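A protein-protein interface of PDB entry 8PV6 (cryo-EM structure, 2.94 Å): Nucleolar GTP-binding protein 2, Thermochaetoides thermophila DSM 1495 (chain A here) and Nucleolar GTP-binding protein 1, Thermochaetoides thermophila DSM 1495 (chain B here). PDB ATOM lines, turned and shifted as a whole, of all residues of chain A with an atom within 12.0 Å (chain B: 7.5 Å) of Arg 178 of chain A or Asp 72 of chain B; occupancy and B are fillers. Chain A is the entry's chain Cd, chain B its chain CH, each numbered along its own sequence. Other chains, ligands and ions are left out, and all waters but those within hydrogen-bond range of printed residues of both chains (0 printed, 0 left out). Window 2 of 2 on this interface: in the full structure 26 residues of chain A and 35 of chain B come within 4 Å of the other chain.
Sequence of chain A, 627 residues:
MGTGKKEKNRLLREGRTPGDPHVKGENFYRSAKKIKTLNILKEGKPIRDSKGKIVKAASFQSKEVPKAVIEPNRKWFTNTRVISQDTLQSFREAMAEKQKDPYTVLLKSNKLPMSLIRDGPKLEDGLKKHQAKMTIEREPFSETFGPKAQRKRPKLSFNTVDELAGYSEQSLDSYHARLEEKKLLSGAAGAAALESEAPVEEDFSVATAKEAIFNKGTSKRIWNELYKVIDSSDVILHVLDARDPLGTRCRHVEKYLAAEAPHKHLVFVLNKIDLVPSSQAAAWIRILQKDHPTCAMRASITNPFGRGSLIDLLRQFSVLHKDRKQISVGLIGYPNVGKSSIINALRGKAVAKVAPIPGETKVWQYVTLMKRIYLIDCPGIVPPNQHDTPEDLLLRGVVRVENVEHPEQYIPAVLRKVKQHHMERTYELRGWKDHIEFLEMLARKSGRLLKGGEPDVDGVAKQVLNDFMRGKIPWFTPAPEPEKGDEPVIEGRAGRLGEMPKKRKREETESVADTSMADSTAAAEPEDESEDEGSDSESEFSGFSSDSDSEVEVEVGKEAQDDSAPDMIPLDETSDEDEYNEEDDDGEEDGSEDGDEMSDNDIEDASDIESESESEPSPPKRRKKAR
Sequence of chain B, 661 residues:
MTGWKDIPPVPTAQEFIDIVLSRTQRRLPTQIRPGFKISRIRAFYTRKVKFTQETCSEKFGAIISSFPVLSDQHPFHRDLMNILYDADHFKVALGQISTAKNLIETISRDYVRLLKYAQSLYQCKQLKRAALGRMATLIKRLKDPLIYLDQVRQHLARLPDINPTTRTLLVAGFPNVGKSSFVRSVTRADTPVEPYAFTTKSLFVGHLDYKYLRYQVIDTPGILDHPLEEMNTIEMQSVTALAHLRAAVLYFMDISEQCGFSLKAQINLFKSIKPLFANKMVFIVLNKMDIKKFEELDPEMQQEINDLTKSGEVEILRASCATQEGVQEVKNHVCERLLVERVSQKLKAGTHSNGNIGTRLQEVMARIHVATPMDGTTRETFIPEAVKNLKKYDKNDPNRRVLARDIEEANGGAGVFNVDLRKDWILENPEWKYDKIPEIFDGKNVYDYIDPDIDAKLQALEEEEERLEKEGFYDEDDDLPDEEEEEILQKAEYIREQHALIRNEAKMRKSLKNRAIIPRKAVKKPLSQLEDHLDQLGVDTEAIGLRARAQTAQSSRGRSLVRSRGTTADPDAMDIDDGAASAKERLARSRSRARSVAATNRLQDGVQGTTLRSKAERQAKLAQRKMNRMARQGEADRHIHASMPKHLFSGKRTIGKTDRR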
ATOM      1  N   TYR A 167      16.070  -2.996  23.831  1.00  0.00           N
ATOM      2  CA  TYR A 167      15.692  -1.590  23.760  1.00  0.00           C
ATOM      3  C   TYR A 167      14.298  -1.427  23.171  1.00  0.00           C
ATOM      4  O   TYR A 167      13.480  -0.661  23.692  1.00  0.00           O
ATOM      5  CB  TYR A 167      16.735  -0.837  22.929  1.00  0.00           C
ATOM      6  CG  TYR A 167      16.338   0.547  22.469  1.00  0.00           C
ATOM      7  CD1 TYR A 167      16.344   0.873  21.120  1.00  0.00           C
ATOM      8  CD2 TYR A 167      15.993   1.535  23.379  1.00  0.00           C
ATOM      9  CE1 TYR A 167      15.993   2.138  20.688  1.00  0.00           C
ATOM     10  CE2 TYR A 167      15.638   2.806  22.958  1.00  0.00           C
ATOM     11  CZ  TYR A 167      15.641   3.100  21.610  1.00  0.00           C
ATOM     12  OH  TYR A 167      15.293   4.360  21.180  1.00  0.00           O
ATOM     13  N   GLU A 169      11.918  -3.715  23.162  1.00  0.00           N
ATOM     14  CA  GLU A 169      10.960  -4.289  24.105  1.00  0.00           C
ATOM     15  C   GLU A 169      10.644  -3.324  25.242  1.00  0.00           C
ATOM     16  O   GLU A 169       9.469  -3.085  25.561  1.00  0.00           O
ATOM     17  CB  GLU A 169      11.500  -5.608  24.657  1.00  0.00           C
ATOM     18  CG  GLU A 169      10.579  -6.290  25.655  1.00  0.00           C
ATOM     19  CD  GLU A 169       9.310  -6.819  25.020  1.00  0.00           C
ATOM     20  OE1 GLU A 169       9.342  -7.176  23.824  1.00  0.00           O
ATOM     21  OE2 GLU A 169       8.277  -6.878  25.720  1.00  0.00           O
ATOM     22  N   GLN A 170      11.677  -2.742  25.858  1.00  0.00           N
ATOM     23  CA  GLN A 170      11.427  -1.852  26.987  1.00  0.00           C
ATOM     24  C   GLN A 170      10.806  -0.541  26.521  1.00  0.00           C
ATOM     25  O   GLN A 170      10.016   0.070  27.249  1.00  0.00           O
ATOM     26  CB  GLN A 170      12.712  -1.612  27.788  1.00  0.00           C
ATOM     27  CG  GLN A 170      13.863  -0.906  27.076  1.00  0.00           C
ATOM     28  CD  GLN A 170      13.738   0.606  27.106  1.00  0.00           C
ATOM     29  OE1 GLN A 170      13.175   1.174  28.042  1.00  0.00           O
ATOM     30  NE2 GLN A 170      14.254   1.264  26.080  1.00  0.00           N
ATOM     31  N   SER A 171      11.133  -0.102  25.299  1.00  0.00           N
ATOM     32  CA  SER A 171      10.515   1.099  24.747  1.00  0.00           C
ATOM     33  C   SER A 171       9.029   0.887  24.504  1.00  0.00           C
ATOM     34  O   SER A 171       8.212   1.766  24.799  1.00  0.00           O
ATOM     35  CB  SER A 171      11.224   1.500  23.454  1.00  0.00           C
ATOM     36  OG  SER A 171      12.567   1.872  23.705  1.00  0.00           O
ATOM     37  N   LEU A 172       8.658  -0.281  23.971  1.00  0.00           N
ATOM     38  CA  LEU A 172       7.244  -0.589  23.777  1.00  0.00           C
ATOM     39  C   LEU A 172       6.512  -0.700  25.108  1.00  0.00           C
ATOM     40  O   LEU A 172       5.371  -0.236  25.235  1.00  0.00           O
ATOM     41  CB  LEU A 172       7.093  -1.879  22.973  1.00  0.00           C
ATOM     42  CG  LEU A 172       5.710  -2.144  22.377  1.00  0.00           C
ATOM     43  CD1 LEU A 172       5.231  -0.946  21.577  1.00  0.00           C
ATOM     44  CD2 LEU A 172       5.735  -3.392  21.513  1.00  0.00           C
ATOM     45  N   ASP A 173       7.155  -1.303  26.114  1.00  0.00           N
ATOM     46  CA  ASP A 173       6.542  -1.409  27.437  1.00  0.00           C
ATOM     47  C   ASP A 173       6.317  -0.032  28.058  1.00  0.00           C
ATOM     48  O   ASP A 173       5.244   0.245  28.610  1.00  0.00           O
ATOM     49  CB  ASP A 173       7.412  -2.273  28.347  1.00  0.00           C
ATOM     50  CG  ASP A 173       6.765  -2.538  29.691  1.00  0.00           C
ATOM     51  OD1 ASP A 173       5.817  -3.349  29.746  1.00  0.00           O
ATOM     52  OD2 ASP A 173       7.203  -1.933  30.691  1.00  0.00           O
ATOM     53  N   SER A 174       7.318   0.849  27.961  1.00  0.00           N
ATOM     54  CA  SER A 174       7.186   2.198  28.504  1.00  0.00           C
ATOM     55  C   SER A 174       6.138   3.003  27.745  1.00  0.00           C
ATOM     56  O   SER A 174       5.390   3.781  28.348  1.00  0.00           O
ATOM     57  CB  SER A 174       8.537   2.909  28.468  1.00  0.00           C
ATOM     58  OG  SER A 174       8.420   4.249  28.913  1.00  0.00           O
ATOM     59  N   TYR A 175       6.073   2.831  26.421  1.00  0.00           N
ATOM     60  CA  TYR A 175       5.077   3.524  25.611  1.00  0.00           C
ATOM     61  C   TYR A 175       3.665   3.091  25.983  1.00  0.00           C
ATOM     62  O   TYR A 175       2.764   3.927  26.130  1.00  0.00           O
ATOM     63  CB  TYR A 175       5.366   3.265  24.131  1.00  0.00           C
ATOM     64  CG  TYR A 175       4.319   3.769  23.168  1.00  0.00           C
ATOM     65  CD1 TYR A 175       3.481   2.885  22.501  1.00  0.00           C
ATOM     66  CD2 TYR A 175       4.179   5.126  22.910  1.00  0.00           C
ATOM     67  CE1 TYR A 175       2.530   3.339  21.611  1.00  0.00           C
ATOM     68  CE2 TYR A 175       3.228   5.589  22.023  1.00  0.00           C
ATOM     69  CZ  TYR A 175       2.407   4.691  21.375  1.00  0.00           C
ATOM     70  OH  TYR A 175       1.459   5.148  20.491  1.00  0.00           O
ATOM     71  N   HIS A 176       3.460   1.781  26.164  1.00  0.00           N
ATOM     72  CA  HIS A 176       2.148   1.287  26.570  1.00  0.00           C
ATOM     73  C   HIS A 176       1.781   1.758  27.973  1.00  0.00           C
ATOM     74  O   HIS A 176       0.625   2.118  28.230  1.00  0.00           O
ATOM     75  CB  HIS A 176       2.111  -0.238  26.487  1.00  0.00           C
ATOM     76  CG  HIS A 176       2.045  -0.763  25.087  1.00  0.00           C
ATOM     77  ND1 HIS A 176       1.207  -0.231  24.132  1.00  0.00           N
ATOM     78  CD2 HIS A 176       2.710  -1.776  24.483  1.00  0.00           C
ATOM     79  CE1 HIS A 176       1.361  -0.891  22.998  1.00  0.00           C
ATOM     80  NE2 HIS A 176       2.266  -1.834  23.184  1.00  0.00           N
ATOM     81  N   ALA A 177       2.753   1.770  28.894  1.00  0.00           N
ATOM     82  CA  ALA A 177       2.486   2.233  30.253  1.00  0.00           C
ATOM     83  C   ALA A 177       2.127   3.716  30.275  1.00  0.00           C
ATOM     84  O   ALA A 177       1.212   4.136  30.993  1.00  0.00           O
ATOM     85  CB  ALA A 177       3.694   1.957  31.147  1.00  0.00           C
ATOM     86  N   ARG A 178       2.834   4.521  29.477  1.00  0.00           N
ATOM     87  CA  ARG A 178       2.527   5.944  29.393  1.00  0.00           C
ATOM     88  C   ARG A 178       1.159   6.183  28.766  1.00  0.00           C
ATOM     89  O   ARG A 178       0.422   7.081  29.193  1.00  0.00           O
ATOM     90  CB  ARG A 178       3.611   6.662  28.594  1.00  0.00           C
ATOM     91  CG  ARG A 178       3.424   8.161  28.498  1.00  0.00           C
ATOM     92  CD  ARG A 178       4.543   8.777  27.692  1.00  0.00           C
ATOM     93  NE  ARG A 178       4.502   8.258  26.331  1.00  0.00           N
ATOM     94  CZ  ARG A 178       3.717   8.726  25.372  1.00  0.00           C
ATOM     95  NH1 ARG A 178       2.920   9.763  25.574  1.00  0.00           N
ATOM     96  NH2 ARG A 178       3.720   8.130  24.183  1.00  0.00           N
ATOM     97  N   LEU A 179       0.802   5.391  27.748  1.00  0.00           N
ATOM     98  CA  LEU A 179      -0.525   5.515  27.149  1.00  0.00           C
ATOM     99  C   LEU A 179      -1.622   5.152  28.141  1.00  0.00           C
ATOM    100  O   LEU A 179      -2.669   5.808  28.184  1.00  0.00           O
ATOM    101  CB  LEU A 179      -0.634   4.646  25.899  1.00  0.00           C
ATOM    102  CG  LEU A 179      -0.018   5.194  24.614  1.00  0.00           C
ATOM    103  CD1 LEU A 179      -0.421   4.318  23.444  1.00  0.00           C
ATOM    104  CD2 LEU A 179      -0.445   6.634  24.384  1.00  0.00           C
ATOM    105  N   GLU A 180      -1.402   4.107  28.944  1.00  0.00           N
ATOM    106  CA  GLU A 180      -2.373   3.758  29.981  1.00  0.00           C
ATOM    107  C   GLU A 180      -2.476   4.856  31.033  1.00  0.00           C
ATOM    108  O   GLU A 180      -3.570   5.138  31.536  1.00  0.00           O
ATOM    109  CB  GLU A 180      -2.006   2.423  30.629  1.00  0.00           C
ATOM    110  CG  GLU A 180      -2.125   1.223  29.701  1.00  0.00           C
ATOM    111  CD  GLU A 180      -3.557   0.930  29.299  1.00  0.00           C
ATOM    112  OE1 GLU A 180      -4.471   1.187  30.110  1.00  0.00           O
ATOM    113  OE2 GLU A 180      -3.769   0.445  28.168  1.00  0.00           O
ATOM    114  N   GLU A 181      -1.350   5.492  31.371  1.00  0.00           N
ATOM    115  CA  GLU A 181      -1.374   6.600  32.324  1.00  0.00           C
ATOM    116  C   GLU A 181      -2.169   7.784  31.780  1.00  0.00           C
ATOM    117  O   GLU A 181      -2.965   8.398  32.502  1.00  0.00           O
ATOM    118  CB  GLU A 181       0.055   7.020  32.670  1.00  0.00           C
ATOM    119  CG  GLU A 181       0.148   8.281  33.515  1.00  0.00           C
ATOM    120  CD  GLU A 181       1.570   8.786  33.653  1.00  0.00           C
ATOM    121  OE1 GLU A 181       2.490   8.128  33.126  1.00  0.00           O
ATOM    122  OE2 GLU A 181       1.767   9.842  34.290  1.00  0.00           O
ATOM    123  N   LYS A 182      -1.972   8.114  30.500  1.00  0.00           N
ATOM    124  CA  LYS A 182      -2.707   9.227  29.901  1.00  0.00           C
ATOM    125  C   LYS A 182      -4.187   8.895  29.741  1.00  0.00           C
ATOM    126  O   LYS A 182      -5.044   9.781  29.830  1.00  0.00           O
ATOM    127  CB  LYS A 182      -2.092   9.613  28.554  1.00  0.00           C
ATOM    128  CG  LYS A 182      -0.624  10.084  28.561  1.00  0.00           C
ATOM    129  CD  LYS A 182      -0.396  11.469  29.191  1.00  0.00           C
ATOM    130  CE  LYS A 182      -0.021  11.425  30.674  1.00  0.00           C
ATOM    131  NZ  LYS A 182       0.292  12.779  31.206  1.00  0.00           N
ATOM    132  N   LYS A 183      -4.507   7.623  29.489  1.00  0.00           N
ATOM    133  CA  LYS A 183      -5.907   7.218  29.397  1.00  0.00           C
ATOM    134  C   LYS A 183      -6.575   7.286  30.766  1.00  0.00           C
ATOM    135  O   LYS A 183      -7.751   7.649  30.879  1.00  0.00           O
ATOM    136  CB  LYS A 183      -6.003   5.814  28.789  1.00  0.00           C
ATOM    137  CG  LYS A 183      -7.421   5.263  28.566  1.00  0.00           C
ATOM    138  CD  LYS A 183      -7.932   4.387  29.711  1.00  0.00           C
ATOM    139  CE  LYS A 183      -7.199   3.059  29.763  1.00  0.00           C
ATOM    140  NZ  LYS A 183      -7.697   2.195  30.869  1.00  0.00           N
ATOM    141  N   LEU A 184      -5.837   6.924  31.820  1.00  0.00           N
ATOM    142  CA  LEU A 184      -6.366   7.037  33.174  1.00  0.00           C
ATOM    143  C   LEU A 184      -6.554   8.496  33.571  1.00  0.00           C
ATOM    144  O   LEU A 184      -7.532   8.846  34.243  1.00  0.00           O
ATOM    145  CB  LEU A 184      -5.439   6.325  34.159  1.00  0.00           C
ATOM    146  CG  LEU A 184      -5.889   6.269  35.620  1.00  0.00           C
ATOM    147  CD1 LEU A 184      -7.280   5.663  35.733  1.00  0.00           C
ATOM    148  CD2 LEU A 184      -4.889   5.488  36.456  1.00  0.00           C
ATOM    149  N   LEU A 185      -5.631   9.362  33.163  1.00  0.00           N
ATOM    150  CA  LEU A 185      -5.742  10.788  33.450  1.00  0.00           C
ATOM    151  C   LEU A 185      -6.820  11.435  32.585  1.00  0.00           C
ATOM    152  O   LEU A 185      -7.214  10.887  31.556  1.00  0.00           O
ATOM    153  CB  LEU A 185      -4.400  11.488  33.228  1.00  0.00           C
ATOM    154  CG  LEU A 185      -4.396  13.006  33.419  1.00  0.00           C
ATOM    155  CD1 LEU A 185      -4.805  13.374  34.837  1.00  0.00           C
ATOM    156  CD2 LEU A 185      -3.031  13.586  33.083  1.00  0.00           C
ATOM    157  N   TRP B   4       2.183  14.002   8.601  1.00  0.00           N
ATOM    158  CA  TRP B   4       2.667  15.268   9.136  1.00  0.00           C
ATOM    159  C   TRP B   4       2.684  16.342   8.057  1.00  0.00           C
ATOM    160  O   TRP B   4       3.554  17.217   8.055  1.00  0.00           O
ATOM    161  CB  TRP B   4       4.052  15.100   9.758  1.00  0.00           C
ATOM    162  CG  TRP B   4       4.120  13.972  10.739  1.00  0.00           C
ATOM    163  CD1 TRP B   4       4.828  12.814  10.607  1.00  0.00           C
ATOM    164  CD2 TRP B   4       3.444  13.886  11.998  1.00  0.00           C
ATOM    165  NE1 TRP B   4       4.640  12.015  11.707  1.00  0.00           N
ATOM    166  CE2 TRP B   4       3.794  12.651  12.576  1.00  0.00           C
ATOM    167  CE3 TRP B   4       2.579  14.736  12.695  1.00  0.00           C
ATOM    168  CZ2 TRP B   4       3.308  12.244  13.815  1.00  0.00           C
ATOM    169  CZ3 TRP B   4       2.100  14.330  13.925  1.00  0.00           C
ATOM    170  CH2 TRP B   4       2.464  13.096  14.473  1.00  0.00           C
ATOM    171  N   PRO B  68       6.006  17.012  15.353  1.00  0.00           N
ATOM    172  CA  PRO B  68       5.752  15.872  16.244  1.00  0.00           C
ATOM    173  C   PRO B  68       6.628  15.913  17.487  1.00  0.00           C
ATOM    174  O   PRO B  68       7.752  16.419  17.468  1.00  0.00           O
ATOM    175  CB  PRO B  68       6.080  14.655  15.370  1.00  0.00           C
ATOM    176  CG  PRO B  68       6.874  15.182  14.231  1.00  0.00           C
ATOM    177  CD  PRO B  68       6.425  16.583  14.010  1.00  0.00           C
ATOM    178  N   VAL B  69       6.093  15.375  18.581  1.00  0.00           N
ATOM    179  CA  VAL B  69       6.823  15.269  19.838  1.00  0.00           C
ATOM    180  C   VAL B  69       7.341  13.837  19.921  1.00  0.00           C
ATOM    181  O   VAL B  69       6.560  12.889  19.942  1.00  0.00           O
ATOM    182  CB  VAL B  69       5.945  15.625  21.036  1.00  0.00           C
ATOM    183  CG1 VAL B  69       6.767  15.596  22.306  1.00  0.00           C
ATOM    184  CG2 VAL B  69       5.304  16.988  20.841  1.00  0.00           C
ATOM    185  N   LEU B  70       8.668  13.688  19.980  1.00  0.00           N
ATOM    186  CA  LEU B  70       9.289  12.368  19.883  1.00  0.00           C
ATOM    187  C   LEU B  70       8.943  11.482  21.072  1.00  0.00           C
ATOM    188  O   LEU B  70       8.811  10.261  20.929  1.00  0.00           O
ATOM    189  CB  LEU B  70      10.805  12.507  19.756  1.00  0.00           C
ATOM    190  CG  LEU B  70      11.402  12.382  18.354  1.00  0.00           C
ATOM    191  CD1 LEU B  70      10.955  13.524  17.473  1.00  0.00           C
ATOM    192  CD2 LEU B  70      12.916  12.325  18.428  1.00  0.00           C
ATOM    193  N   SER B  71       8.795  12.078  22.257  1.00  0.00           N
ATOM    194  CA  SER B  71       8.501  11.291  23.449  1.00  0.00           C
ATOM    195  C   SER B  71       7.093  10.709  23.419  1.00  0.00           C
ATOM    196  O   SER B  71       6.816   9.725  24.114  1.00  0.00           O
ATOM    197  CB  SER B  71       8.692  12.149  24.699  1.00  0.00           C
ATOM    198  OG  SER B  71      10.044  12.550  24.836  1.00  0.00           O
ATOM    199  N   ASP B  72       6.194  11.293  22.629  1.00  0.00           N
ATOM    200  CA  ASP B  72       4.811  10.843  22.559  1.00  0.00           C
ATOM    201  C   ASP B  72       4.511  10.012  21.317  1.00  0.00           C
ATOM    202  O   ASP B  72       3.343   9.707  21.061  1.00  0.00           O
ATOM    203  CB  ASP B  72       3.862  12.038  22.630  1.00  0.00           C
ATOM    204  CG  ASP B  72       4.016  12.825  23.916  1.00  0.00           C
ATOM    205  OD1 ASP B  72       3.075  12.810  24.738  1.00  0.00           O
ATOM    206  OD2 ASP B  72       5.076  13.451  24.112  1.00  0.00           O
ATOM    207  N   GLN B  73       5.524   9.645  20.541  1.00  0.00           N
ATOM    208  CA  GLN B  73       5.316   8.818  19.362  1.00  0.00           C
ATOM    209  C   GLN B  73       5.449   7.342  19.702  1.00  0.00           C
ATOM    210  O   GLN B  73       5.883   6.967  20.794  1.00  0.00           O
ATOM    211  CB  GLN B  73       6.310   9.169  18.254  1.00  0.00           C
ATOM    212  CG  GLN B  73       6.213  10.586  17.754  1.00  0.00           C
ATOM    213  CD  GLN B  73       4.984  10.818  16.908  1.00  0.00           C
ATOM    214  OE1 GLN B  73       4.453   9.893  16.297  1.00  0.00           O
ATOM    215  NE2 GLN B  73       4.514  12.056  16.882  1.00  0.00           N
ATOM    216  N   HIS B  74       5.057   6.508  18.747  1.00  0.00           N
ATOM    217  CA  HIS B  74       5.359   5.089  18.823  1.00  0.00           C
ATOM    218  C   HIS B  74       6.871   4.904  18.725  1.00  0.00           C
ATOM    219  O   HIS B  74       7.551   5.734  18.111  1.00  0.00           O
ATOM    220  CB  HIS B  74       4.643   4.348  17.690  1.00  0.00           C
ATOM    221  CG  HIS B  74       4.685   2.857  17.808  1.00  0.00           C
ATOM    222  ND1 HIS B  74       5.730   2.101  17.327  1.00  0.00           N
ATOM    223  CD2 HIS B  74       3.809   1.983  18.356  1.00  0.00           C
ATOM    224  CE1 HIS B  74       5.496   0.824  17.572  1.00  0.00           C
ATOM    225  NE2 HIS B  74       4.337   0.725  18.195  1.00  0.00           N
ATOM    226  N   PRO B  75       7.437   3.866  19.358  1.00  0.00           N
ATOM    227  CA  PRO B  75       8.894   3.654  19.269  1.00  0.00           C
ATOM    228  C   PRO B  75       9.422   3.495  17.851  1.00  0.00           C
ATOM    229  O   PRO B  75      10.557   3.908  17.574  1.00  0.00           O
ATOM    230  CB  PRO B  75       9.099   2.378  20.092  1.00  0.00           C
ATOM    231  CG  PRO B  75       8.021   2.423  21.102  1.00  0.00           C
ATOM    232  CD  PRO B  75       6.837   3.074  20.446  1.00  0.00           C
ATOM    233  N   ARG B  78       9.513   7.130  16.517  1.00  0.00           N
ATOM    234  CA  ARG B  78      10.562   7.863  17.221  1.00  0.00           C
ATOM    235  C   ARG B  78      11.949   7.450  16.744  1.00  0.00           C
ATOM    236  O   ARG B  78      12.790   8.305  16.438  1.00  0.00           O
ATOM    237  CB  ARG B  78      10.425   7.638  18.725  1.00  0.00           C
ATOM    238  CG  ARG B  78      11.543   8.242  19.551  1.00  0.00           C
ATOM    239  CD  ARG B  78      11.279   8.064  21.041  1.00  0.00           C
ATOM    240  NE  ARG B  78      10.977   6.682  21.398  1.00  0.00           N
ATOM    241  CZ  ARG B  78      11.867   5.699  21.453  1.00  0.00           C
ATOM    242  NH1 ARG B  78      13.152   5.910  21.221  1.00  0.00           N
ATOM    243  NH2 ARG B  78      11.457   4.471  21.759  1.00  0.00           N
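The guanidinium group (NH2) of Arg 178 of chain A sits at hydrogen-bond distance from the backbone carbonyl oxygen (O) of Ser 71 of chain B, at 3.5 Å. The side-chain hydroxyl of Tyr 167 of chain A sits at hydrogen-bond distance from the guanidinium group of Arg 78 of chain B (2.6 Å). NH1 of Arg 178 of chain A is in salt-bridge range of OD1 of Asp 72 of chain B. NH2 of Arg 78 of chain B lies close to OG of Ser 171 of chain A, at 3.4 Å.
Among the printed residues, pairs that only touch across the chains: Ser 171 of chain A with Pro 75 of chain B (3.8 Å), Leu 172 of chain A with His 74 of chain B (3.9 Å), Leu 172 of chain A with Pro 75 of chain B (3.99 Å), Tyr 175 of chain A with Gln 73 of chain B (3.2 Å), Tyr 175 of chain A with His 74 of chain B (3.8 Å) and Tyr 175 of chain A with Pro 75 of chain B (3.8 Å).
The backbone carbonyl oxygen (O) of Tyr 167 of chain A lies within hydrogen-bond range of the side-chain hydroxyl (OG) of Ser 171 of chain A, 2.7 Å away. The backbone carbonyl oxygen (O) of Tyr 167 of chain A lies within hydrogen-bond range of the side-chain amide nitrogen (NE2) of Gln 170 of chain A (3.2 Å). The side-chain hydroxyl (OG) of Ser 171 of chain A lies within hydrogen-bond range of the side-chain amide nitrogen (NE2) of Gln 170 of chain A, at 3.0 Å.
Printed residues of chain A that touch a printed residue of chain B: Tyr 167, Ser 171, Leu 172, Tyr 175 and Arg 178. Hydrophobic or aromatic side chains of chain A within 4 Å of the printed part of chain B: Tyr 167, Leu 172 and Tyr 175. Along chain A the printed residues that touch a printed residue of chain B span positions 167 to 178. Hydrophobic or aromatic side chains of chain B that line the printed part of chain A: His 74 and Pro 75. Among the printed residues, 10 pairs touch across the chains. Among the printed residues, Asp or Glu carboxylates within 4 Å of a Lys or Arg side-chain nitrogen of the other chain: Arg 178 of chain A with Asp 72 of chain B (3.2 Å).
Glu 169 of chain A touches none of the printed residues of chain B. Printed residues of chain B within 4 Å of Leu 172 of chain A: His 74 and Pro 75. Of the printed residues of chain B, Tyr 175 of chain A touches Gln 73, His 74 and Pro 75. No residue of chain B comes within 4 Å of Ala 177 of chain A. No residue of chain A comes within 4 Å of Val 69 of chain B. Ser 71 of chain B touches one residue of chain A. Of the printed residues of chain A, Asp 72 of chain B touches Arg 178 (3.2 Å). Of the printed residues of chain A, Gln 73 of chain B touches Tyr 175. Of the printed residues of chain A, His 74 of chain B touches Leu 172 (3.9 Å) and Tyr 175 (3.8 Å). The nearest residue of chain B that does not touch Arg 178 of chain A is Gln 73 of chain B (4.2 Å).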
